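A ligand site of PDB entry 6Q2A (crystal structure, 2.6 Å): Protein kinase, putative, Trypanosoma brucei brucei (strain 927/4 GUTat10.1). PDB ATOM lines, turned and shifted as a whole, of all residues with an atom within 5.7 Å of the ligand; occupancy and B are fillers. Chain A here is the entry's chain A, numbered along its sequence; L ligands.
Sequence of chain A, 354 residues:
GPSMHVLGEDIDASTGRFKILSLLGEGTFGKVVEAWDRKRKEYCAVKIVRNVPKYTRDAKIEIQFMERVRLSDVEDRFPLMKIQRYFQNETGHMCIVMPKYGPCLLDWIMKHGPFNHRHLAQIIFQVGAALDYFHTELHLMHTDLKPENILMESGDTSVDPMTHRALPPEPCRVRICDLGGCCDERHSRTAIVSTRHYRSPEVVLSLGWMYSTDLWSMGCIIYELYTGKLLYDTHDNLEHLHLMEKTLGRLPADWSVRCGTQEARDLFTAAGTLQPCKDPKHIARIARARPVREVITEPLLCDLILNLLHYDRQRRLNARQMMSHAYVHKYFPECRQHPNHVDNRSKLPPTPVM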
ATOM      1  N   LEU A  24      -7.752  16.146  17.950  1.00  0.00           N
ATOM      2  CA  LEU A  24      -9.132  15.698  18.003  1.00  0.00           C
ATOM      3  C   LEU A  24      -9.293  14.216  17.691  1.00  0.00           C
ATOM      4  O   LEU A  24     -10.208  13.568  18.214  1.00  0.00           O
ATOM      5  CB  LEU A  24      -9.987  16.536  17.059  1.00  0.00           C
ATOM      6  CG  LEU A  24      -9.970  18.030  17.414  1.00  0.00           C
ATOM      7  CD1 LEU A  24     -10.245  18.871  16.185  1.00  0.00           C
ATOM      8  CD2 LEU A  24     -10.984  18.334  18.524  1.00  0.00           C
ATOM      9  N   GLY A  25      -8.428  13.678  16.841  1.00  0.00           N
ATOM     10  CA  GLY A  25      -8.490  12.277  16.491  1.00  0.00           C
ATOM     11  C   GLY A  25      -7.300  11.886  15.661  1.00  0.00           C
ATOM     12  O   GLY A  25      -6.605  12.732  15.082  1.00  0.00           O
ATOM     13  N   GLU A  26      -7.063  10.584  15.608  1.00  0.00           N
ATOM     14  CA  GLU A  26      -5.863  10.039  14.998  1.00  0.00           C
ATOM     15  C   GLU A  26      -6.177   8.695  14.358  1.00  0.00           C
ATOM     16  O   GLU A  26      -7.008   7.945  14.867  1.00  0.00           O
ATOM     17  CB  GLU A  26      -4.742   9.900  16.038  1.00  0.00           C
ATOM     18  CG  GLU A  26      -3.409   9.417  15.484  1.00  0.00           C
ATOM     19  CD  GLU A  26      -2.354   9.334  16.567  1.00  0.00           C
ATOM     20  OE1 GLU A  26      -1.277   8.760  16.309  1.00  0.00           O
ATOM     21  OE2 GLU A  26      -2.611   9.826  17.687  1.00  0.00           O
ATOM     22  N   PHE A  29      -4.924   7.254   8.316  1.00  0.00           N
ATOM     23  CA  PHE A  29      -4.870   8.397   7.402  1.00  0.00           C
ATOM     24  C   PHE A  29      -3.894   9.464   7.901  1.00  0.00           C
ATOM     25  O   PHE A  29      -3.168  10.068   7.109  1.00  0.00           O
ATOM     26  CB  PHE A  29      -6.261   9.014   7.256  1.00  0.00           C
ATOM     27  CG  PHE A  29      -6.780   9.632   8.524  1.00  0.00           C
ATOM     28  CD1 PHE A  29      -7.343   8.851   9.511  1.00  0.00           C
ATOM     29  CD2 PHE A  29      -6.663  10.997   8.743  1.00  0.00           C
ATOM     30  CE1 PHE A  29      -7.810   9.407  10.686  1.00  0.00           C
ATOM     31  CE2 PHE A  29      -7.118  11.572   9.918  1.00  0.00           C
ATOM     32  CZ  PHE A  29      -7.695  10.774  10.895  1.00  0.00           C
ATOM     33  N   VAL A  32      -6.501  14.566  12.796  1.00  0.00           N
ATOM     34  CA  VAL A  32      -7.383  15.729  12.731  1.00  0.00           C
ATOM     35  C   VAL A  32      -7.098  16.586  13.967  1.00  0.00           C
ATOM     36  O   VAL A  32      -7.239  16.102  15.104  1.00  0.00           O
ATOM     37  CB  VAL A  32      -8.862  15.329  12.667  1.00  0.00           C
ATOM     38  CG1 VAL A  32      -9.724  16.565  12.435  1.00  0.00           C
ATOM     39  CG2 VAL A  32      -9.086  14.299  11.575  1.00  0.00           C
ATOM     40  N   ALA A  45     -10.817  22.671  12.013  1.00  0.00           N
ATOM     41  CA  ALA A  45     -10.255  21.337  12.063  1.00  0.00           C
ATOM     42  C   ALA A  45      -9.377  21.140  10.845  1.00  0.00           C
ATOM     43  O   ALA A  45      -9.768  21.478   9.720  1.00  0.00           O
ATOM     44  CB  ALA A  45     -11.369  20.281  12.113  1.00  0.00           C
ATOM     45  N   LYS A  47      -7.136  18.279   8.756  1.00  0.00           N
ATOM     46  CA  LYS A  47      -6.783  16.889   8.499  1.00  0.00           C
ATOM     47  C   LYS A  47      -5.361  16.855   7.931  1.00  0.00           C
ATOM     48  O   LYS A  47      -5.119  17.352   6.827  1.00  0.00           O
ATOM     49  CB  LYS A  47      -7.788  16.275   7.535  1.00  0.00           C
ATOM     50  CG  LYS A  47      -7.552  14.814   7.206  1.00  0.00           C
ATOM     51  CD  LYS A  47      -8.641  14.321   6.270  1.00  0.00           C
ATOM     52  CE  LYS A  47      -8.577  12.817   6.073  1.00  0.00           C
ATOM     53  NZ  LYS A  47      -9.579  12.383   5.067  1.00  0.00           N
ATOM     54  N   MET A  81     -19.909  17.554   4.196  1.00  0.00           N
ATOM     55  CA  MET A  81     -18.760  18.312   4.668  1.00  0.00           C
ATOM     56  C   MET A  81     -18.396  19.398   3.671  1.00  0.00           C
ATOM     57  O   MET A  81     -18.567  19.244   2.458  1.00  0.00           O
ATOM     58  CB  MET A  81     -17.609  17.332   4.885  1.00  0.00           C
ATOM     59  CG  MET A  81     -16.225  17.861   5.135  1.00  0.00           C
ATOM     60  SD  MET A  81     -15.072  16.560   4.613  1.00  0.00           S
ATOM     61  CE  MET A  81     -14.291  16.099   6.165  1.00  0.00           C
ATOM     62  N   MET A  98     -10.962  22.576   7.369  1.00  0.00           N
ATOM     63  CA  MET A  98     -12.400  22.407   7.367  1.00  0.00           C
ATOM     64  C   MET A  98     -12.976  23.042   8.629  1.00  0.00           C
ATOM     65  O   MET A  98     -12.214  23.389   9.536  1.00  0.00           O
ATOM     66  CB  MET A  98     -12.758  20.921   7.291  1.00  0.00           C
ATOM     67  CG  MET A  98     -12.540  20.299   5.929  1.00  0.00           C
ATOM     68  SD  MET A  98     -12.860  18.543   5.996  1.00  0.00           S
ATOM     69  CE  MET A  98     -11.319  17.922   6.660  1.00  0.00           C
ATOM     70  N   PRO A  99     -14.291  23.210   8.743  1.00  0.00           N
ATOM     71  CA  PRO A  99     -14.860  23.642  10.021  1.00  0.00           C
ATOM     72  C   PRO A  99     -14.662  22.569  11.070  1.00  0.00           C
ATOM     73  O   PRO A  99     -14.435  21.396  10.761  1.00  0.00           O
ATOM     74  CB  PRO A  99     -16.346  23.846   9.710  1.00  0.00           C
ATOM     75  CG  PRO A  99     -16.451  23.884   8.216  1.00  0.00           C
ATOM     76  CD  PRO A  99     -15.336  23.034   7.707  1.00  0.00           C
ATOM     77  N   LYS A 100     -14.739  22.983  12.326  1.00  0.00           N
ATOM     78  CA  LYS A 100     -14.621  22.050  13.437  1.00  0.00           C
ATOM     79  C   LYS A 100     -16.011  21.504  13.724  1.00  0.00           C
ATOM     80  O   LYS A 100     -16.909  22.250  14.119  1.00  0.00           O
ATOM     81  CB  LYS A 100     -14.017  22.711  14.667  1.00  0.00           C
ATOM     82  CG  LYS A 100     -13.642  21.724  15.778  1.00  0.00           C
ATOM     83  CD  LYS A 100     -13.504  22.417  17.120  1.00  0.00           C
ATOM     84  CE  LYS A 100     -13.584  21.408  18.258  1.00  0.00           C
ATOM     85  NZ  LYS A 100     -13.833  22.074  19.572  1.00  0.00           N
ATOM     86  N   TYR A 101     -16.193  20.208  13.509  1.00  0.00           N
ATOM     87  CA  TYR A 101     -17.449  19.559  13.803  1.00  0.00           C
ATOM     88  C   TYR A 101     -17.282  18.794  15.128  1.00  0.00           C
ATOM     89  O   TYR A 101     -16.335  19.044  15.876  1.00  0.00           O
ATOM     90  CB  TYR A 101     -17.858  18.647  12.634  1.00  0.00           C
ATOM     91  CG  TYR A 101     -18.090  19.384  11.317  1.00  0.00           C
ATOM     92  CD1 TYR A 101     -18.824  20.558  11.265  1.00  0.00           C
ATOM     93  CD2 TYR A 101     -17.572  18.875  10.119  1.00  0.00           C
ATOM     94  CE1 TYR A 101     -19.031  21.215  10.063  1.00  0.00           C
ATOM     95  CE2 TYR A 101     -17.779  19.533   8.918  1.00  0.00           C
ATOM     96  CZ  TYR A 101     -18.507  20.702   8.895  1.00  0.00           C
ATOM     97  OH  TYR A 101     -18.712  21.358   7.703  1.00  0.00           O
ATOM     98  N   GLY A 102     -18.190  17.884  15.419  1.00  0.00           N
ATOM     99  CA  GLY A 102     -18.135  17.111  16.632  1.00  0.00           C
ATOM    100  C   GLY A 102     -17.661  15.701  16.398  1.00  0.00           C
ATOM    101  O   GLY A 102     -17.085  15.373  15.354  1.00  0.00           O
ATOM    102  N   PRO A 103     -17.898  14.826  17.374  1.00  0.00           N
ATOM    103  CA  PRO A 103     -17.491  13.424  17.227  1.00  0.00           C
ATOM    104  C   PRO A 103     -18.465  12.675  16.338  1.00  0.00           C
ATOM    105  O   PRO A 103     -19.604  13.094  16.106  1.00  0.00           O
ATOM    106  CB  PRO A 103     -17.512  12.888  18.662  1.00  0.00           C
ATOM    107  CG  PRO A 103     -18.084  14.009  19.530  1.00  0.00           C
ATOM    108  CD  PRO A 103     -18.643  15.059  18.613  1.00  0.00           C
ATOM    109  N   CYS A 104     -17.983  11.546  15.808  1.00  0.00           N
ATOM    110  CA  CYS A 104     -18.792  10.673  14.977  1.00  0.00           C
ATOM    111  C   CYS A 104     -19.949  10.064  15.785  1.00  0.00           C
ATOM    112  O   CYS A 104     -19.960  10.094  17.014  1.00  0.00           O
ATOM    113  CB  CYS A 104     -17.939   9.575  14.345  1.00  0.00           C
ATOM    114  SG  CYS A 104     -17.090   8.494  15.497  1.00  0.00           S
ATOM    115  N   LEU A 106     -20.474   6.963  16.048  1.00  0.00           N
ATOM    116  CA  LEU A 106     -19.958   5.819  16.792  1.00  0.00           C
ATOM    117  C   LEU A 106     -19.565   6.220  18.208  1.00  0.00           C
ATOM    118  O   LEU A 106     -19.794   5.465  19.161  1.00  0.00           O
ATOM    119  CB  LEU A 106     -18.775   5.204  16.060  1.00  0.00           C
ATOM    120  CG  LEU A 106     -18.194   3.938  16.698  1.00  0.00           C
ATOM    121  CD1 LEU A 106     -19.109   2.737  16.454  1.00  0.00           C
ATOM    122  CD2 LEU A 106     -16.779   3.655  16.192  1.00  0.00           C
ATOM    123  N   ASP A 107     -18.941   7.383  18.370  1.00  0.00           N
ATOM    124  CA  ASP A 107     -18.575   7.853  19.700  1.00  0.00           C
ATOM    125  C   ASP A 107     -19.800   8.041  20.585  1.00  0.00           C
ATOM    126  O   ASP A 107     -19.762   7.738  21.789  1.00  0.00           O
ATOM    127  CB  ASP A 107     -17.763   9.143  19.597  1.00  0.00           C
ATOM    128  CG  ASP A 107     -16.337   8.890  19.136  1.00  0.00           C
ATOM    129  OD1 ASP A 107     -16.020   7.734  18.780  1.00  0.00           O
ATOM    130  OD2 ASP A 107     -15.538   9.850  19.114  1.00  0.00           O
ATOM    131  N   MET A 110     -21.464   4.584  21.726  1.00  0.00           N
ATOM    132  CA  MET A 110     -20.670   3.828  22.676  1.00  0.00           C
ATOM    133  C   MET A 110     -20.691   4.460  24.071  1.00  0.00           C
ATOM    134  O   MET A 110     -20.536   3.737  25.065  1.00  0.00           O
ATOM    135  CB  MET A 110     -19.247   3.684  22.161  1.00  0.00           C
ATOM    136  CG  MET A 110     -19.183   2.816  20.923  1.00  0.00           C
ATOM    137  SD  MET A 110     -17.719   1.784  20.798  1.00  0.00           S
ATOM    138  CE  MET A 110     -16.662   2.812  19.782  1.00  0.00           C
ATOM    139  N   PRO A 147     -20.558   4.636  10.627  1.00  0.00           N
ATOM    140  CA  PRO A 147     -20.742   5.498  11.806  1.00  0.00           C
ATOM    141  C   PRO A 147     -19.511   6.303  12.197  1.00  0.00           C
ATOM    142  O   PRO A 147     -19.649   7.303  12.913  1.00  0.00           O
ATOM    143  CB  PRO A 147     -21.142   4.507  12.899  1.00  0.00           C
ATOM    144  CG  PRO A 147     -21.727   3.341  12.169  1.00  0.00           C
ATOM    145  CD  PRO A 147     -20.922   3.236  10.899  1.00  0.00           C
ATOM    146  N   GLU A 148     -18.315   5.909  11.759  1.00  0.00           N
ATOM    147  CA  GLU A 148     -17.104   6.626  12.128  1.00  0.00           C
ATOM    148  C   GLU A 148     -16.908   7.904  11.322  1.00  0.00           C
ATOM    149  O   GLU A 148     -16.154   8.785  11.772  1.00  0.00           O
ATOM    150  CB  GLU A 148     -15.860   5.755  11.951  1.00  0.00           C
ATOM    151  CG  GLU A 148     -15.824   4.490  12.804  1.00  0.00           C
ATOM    152  CD  GLU A 148     -16.414   3.296  12.081  1.00  0.00           C
ATOM    153  OE1 GLU A 148     -17.582   3.367  11.671  1.00  0.00           O
ATOM    154  OE2 GLU A 148     -15.693   2.281  11.925  1.00  0.00           O
ATOM    155  N   LEU A 151     -20.374  12.571  11.310  1.00  0.00           N
ATOM    156  CA  LEU A 151     -19.975  13.346  12.478  1.00  0.00           C
ATOM    157  C   LEU A 151     -21.164  14.176  12.947  1.00  0.00           C
ATOM    158  O   LEU A 151     -21.940  14.676  12.137  1.00  0.00           O
ATOM    159  CB  LEU A 151     -18.812  14.279  12.169  1.00  0.00           C
ATOM    160  CG  LEU A 151     -17.516  13.719  11.600  1.00  0.00           C
ATOM    161  CD1 LEU A 151     -16.431  14.780  11.640  1.00  0.00           C
ATOM    162  CD2 LEU A 151     -17.089  12.472  12.355  1.00  0.00           C
ATOM    163  N   CYS A 177     -18.787  12.776   6.059  1.00  0.00           N
ATOM    164  CA  CYS A 177     -17.369  13.034   5.832  1.00  0.00           C
ATOM    165  C   CYS A 177     -16.746  11.962   4.941  1.00  0.00           C
ATOM    166  O   CYS A 177     -17.435  11.124   4.350  1.00  0.00           O
ATOM    167  CB  CYS A 177     -16.602  13.060   7.158  1.00  0.00           C
ATOM    168  SG  CYS A 177     -16.848  14.484   8.207  1.00  0.00           S
ATOM    169  N   ASP A 178     -15.424  12.034   4.836  1.00  0.00           N
ATOM    170  CA  ASP A 178     -14.573  11.017   4.208  1.00  0.00           C
ATOM    171  C   ASP A 178     -15.029  10.699   2.788  1.00  0.00           C
ATOM    172  O   ASP A 178     -15.613   9.644   2.501  1.00  0.00           O
ATOM    173  CB  ASP A 178     -14.496   9.769   5.087  1.00  0.00           C
ATOM    174  CG  ASP A 178     -13.418   9.874   6.145  1.00  0.00           C
ATOM    175  OD1 ASP A 178     -12.743  10.934   6.187  1.00  0.00           O
ATOM    176  OD2 ASP A 178     -13.234   8.916   6.938  1.00  0.00           O
HETATM  177  C1  LIG L   1     -13.898   5.659  17.813  1.00  0.00           C
HETATM  178  C2  LIG L   1     -14.661   7.118  16.066  1.00  0.00           C
HETATM  179  C3  LIG L   1     -15.280   8.457  15.718  1.00  0.00           C
HETATM  180  O1  LIG L   1     -14.374  18.102  13.314  1.00  0.00           O
HETATM  181  O2  LIG L   1     -15.426  11.199  15.843  1.00  0.00           O
HETATM  182  C4  LIG L   1     -13.661  16.013  15.160  1.00  0.00           C
HETATM  183  C5  LIG L   1     -13.837  17.067  12.944  1.00  0.00           C
HETATM  184  C6  LIG L   1     -13.624  16.765  11.492  1.00  0.00           C
HETATM  185  C7  LIG L   1     -14.009  17.652  10.501  1.00  0.00           C
HETATM  186  C8  LIG L   1     -13.780  17.308   9.185  1.00  0.00           C
HETATM  187  C9  LIG L   1     -12.832  15.295   9.764  1.00  0.00           C
HETATM  188  C10 LIG L   1     -12.210  14.010   9.313  1.00  0.00           C
HETATM  189  C11 LIG L   1     -13.025  15.566  11.113  1.00  0.00           C
HETATM  190  C12 LIG L   1     -14.238  16.540  17.160  1.00  0.00           C
HETATM  191  C13 LIG L   1     -14.741  17.185  18.285  1.00  0.00           C
HETATM  192  C14 LIG L   1     -14.914  16.449  19.447  1.00  0.00           C
HETATM  193  C15 LIG L   1     -14.589  15.098  19.492  1.00  0.00           C
HETATM  194  C16 LIG L   1     -14.071  14.448  18.374  1.00  0.00           C
HETATM  195  C17 LIG L   1     -13.707  12.984  18.474  1.00  0.00           C
HETATM  196  C18 LIG L   1     -13.900  15.186  17.201  1.00  0.00           C
HETATM  197  C19 LIG L   1     -14.170  13.061  14.286  1.00  0.00           C
HETATM  198  C20 LIG L   1     -12.803   7.756  17.469  1.00  0.00           C
HETATM  199  C21 LIG L   1     -14.688  10.787  14.958  1.00  0.00           C
HETATM  200  C22 LIG L   1     -14.385   9.307  14.829  1.00  0.00           C
HETATM  201  N1  LIG L   1     -14.085   7.052  17.406  1.00  0.00           N
HETATM  202  N2  LIG L   1     -14.111  11.619  14.070  1.00  0.00           N
HETATM  203  C23 LIG L   1     -13.148  13.540  15.296  1.00  0.00           C
HETATM  204  C24 LIG L   1     -11.714  13.454  14.768  1.00  0.00           C
HETATM  205  C25 LIG L   1     -11.317  12.181  14.034  1.00  0.00           C
HETATM  206  C26 LIG L   1     -12.039  11.913  12.730  1.00  0.00           C
HETATM  207  C27 LIG L   1     -13.356  11.170  12.896  1.00  0.00           C
HETATM  208  N3  LIG L   1     -13.536  14.851  15.879  1.00  0.00           N
HETATM  209  N4  LIG L   1     -14.069  17.049  15.866  1.00  0.00           N
HETATM  210  N5  LIG L   1     -13.376  16.113  13.825  1.00  0.00           N
HETATM  211  N6  LIG L   1     -13.214  16.163   8.800  1.00  0.00           N
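The side-chain sulfur (SD) of Met 98 lies close to a nitrogen (N6) of the ligand (3.7 Å).
A nitrogen (N4) of the ligand lies close to the backbone carbonyl oxygen (O) of Gly 102 (3.5 Å).
Leu 24 touches the ligand (O to C17, 3.6 Å).
CA of Gly 25 touches C25 of the ligand, at 3.7 Å.
CG1 of Val 32 touches C11 of the ligand, at 3.7 Å.
Ala 45 touches the ligand (CB to O1, 3.9 Å).
CE of Met 81 touches N6 of the ligand, at 2.8 Å.
Pro 99 touches the ligand.
Lys 100 touches the ligand (C to O1, 3.8 Å).
CA of Pro 103 touches O2 of the ligand, 3.3 Å away.
Leu 106 touches the ligand (CD2 to C1, 3.9 Å).
Glu 148 touches the ligand (O to C22, 3.6 Å).
Leu 151 touches the ligand (CD1 to C6, 3.4 Å).
Hydrophobic or aromatic side chains within 4 Å of the ligand: Leu 24, Val 32, Ala 45, Met 81, Met 98, Tyr 101, Pro 103, Leu 106 and Leu 151.
The nearest printed residue that does not touch the ligand is Cys 177 (4.05 Å).
SG of Cys 104 sits at hydrogen-bond distance from N of Asp 107 (3.6 Å).
The side-chain sulfur (SG) of Cys 104 lies close to the backbone NH (N) of Leu 106 (3.8 Å).
N of Met 98 is in hydrogen-bond range of O of Ala 45.
The backbone carbonyl oxygen (O) of Val 32 sits at hydrogen-bond distance from the backbone NH (N) of Leu 24, at 2.9 Å.
The backbone NH (N) of Val 32 sits at hydrogen-bond distance from the backbone carbonyl oxygen (O) of Gly 25, 2.9 Å away.
The backbone NH (N) of Leu 106 lies within hydrogen-bond range of the backbone carbonyl oxygen (O) of Pro 147 (3.3 Å).
N of Cys 104 lies within hydrogen-bond range of O2 of the ligand (2.6 Å).
A carbon (C3) of the ligand is covalently linked to the side-chain sulfur (SG) of Cys 104, at 1.8 Å.
The side-chain carboxylate (OD1) of Asp 107 lies within salt-bridge range of a nitrogen (N1) of the ligand, 2.5 Å away.
O1 of the ligand is in hydrogen-bond range of N of Tyr 101 (2.8 Å).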
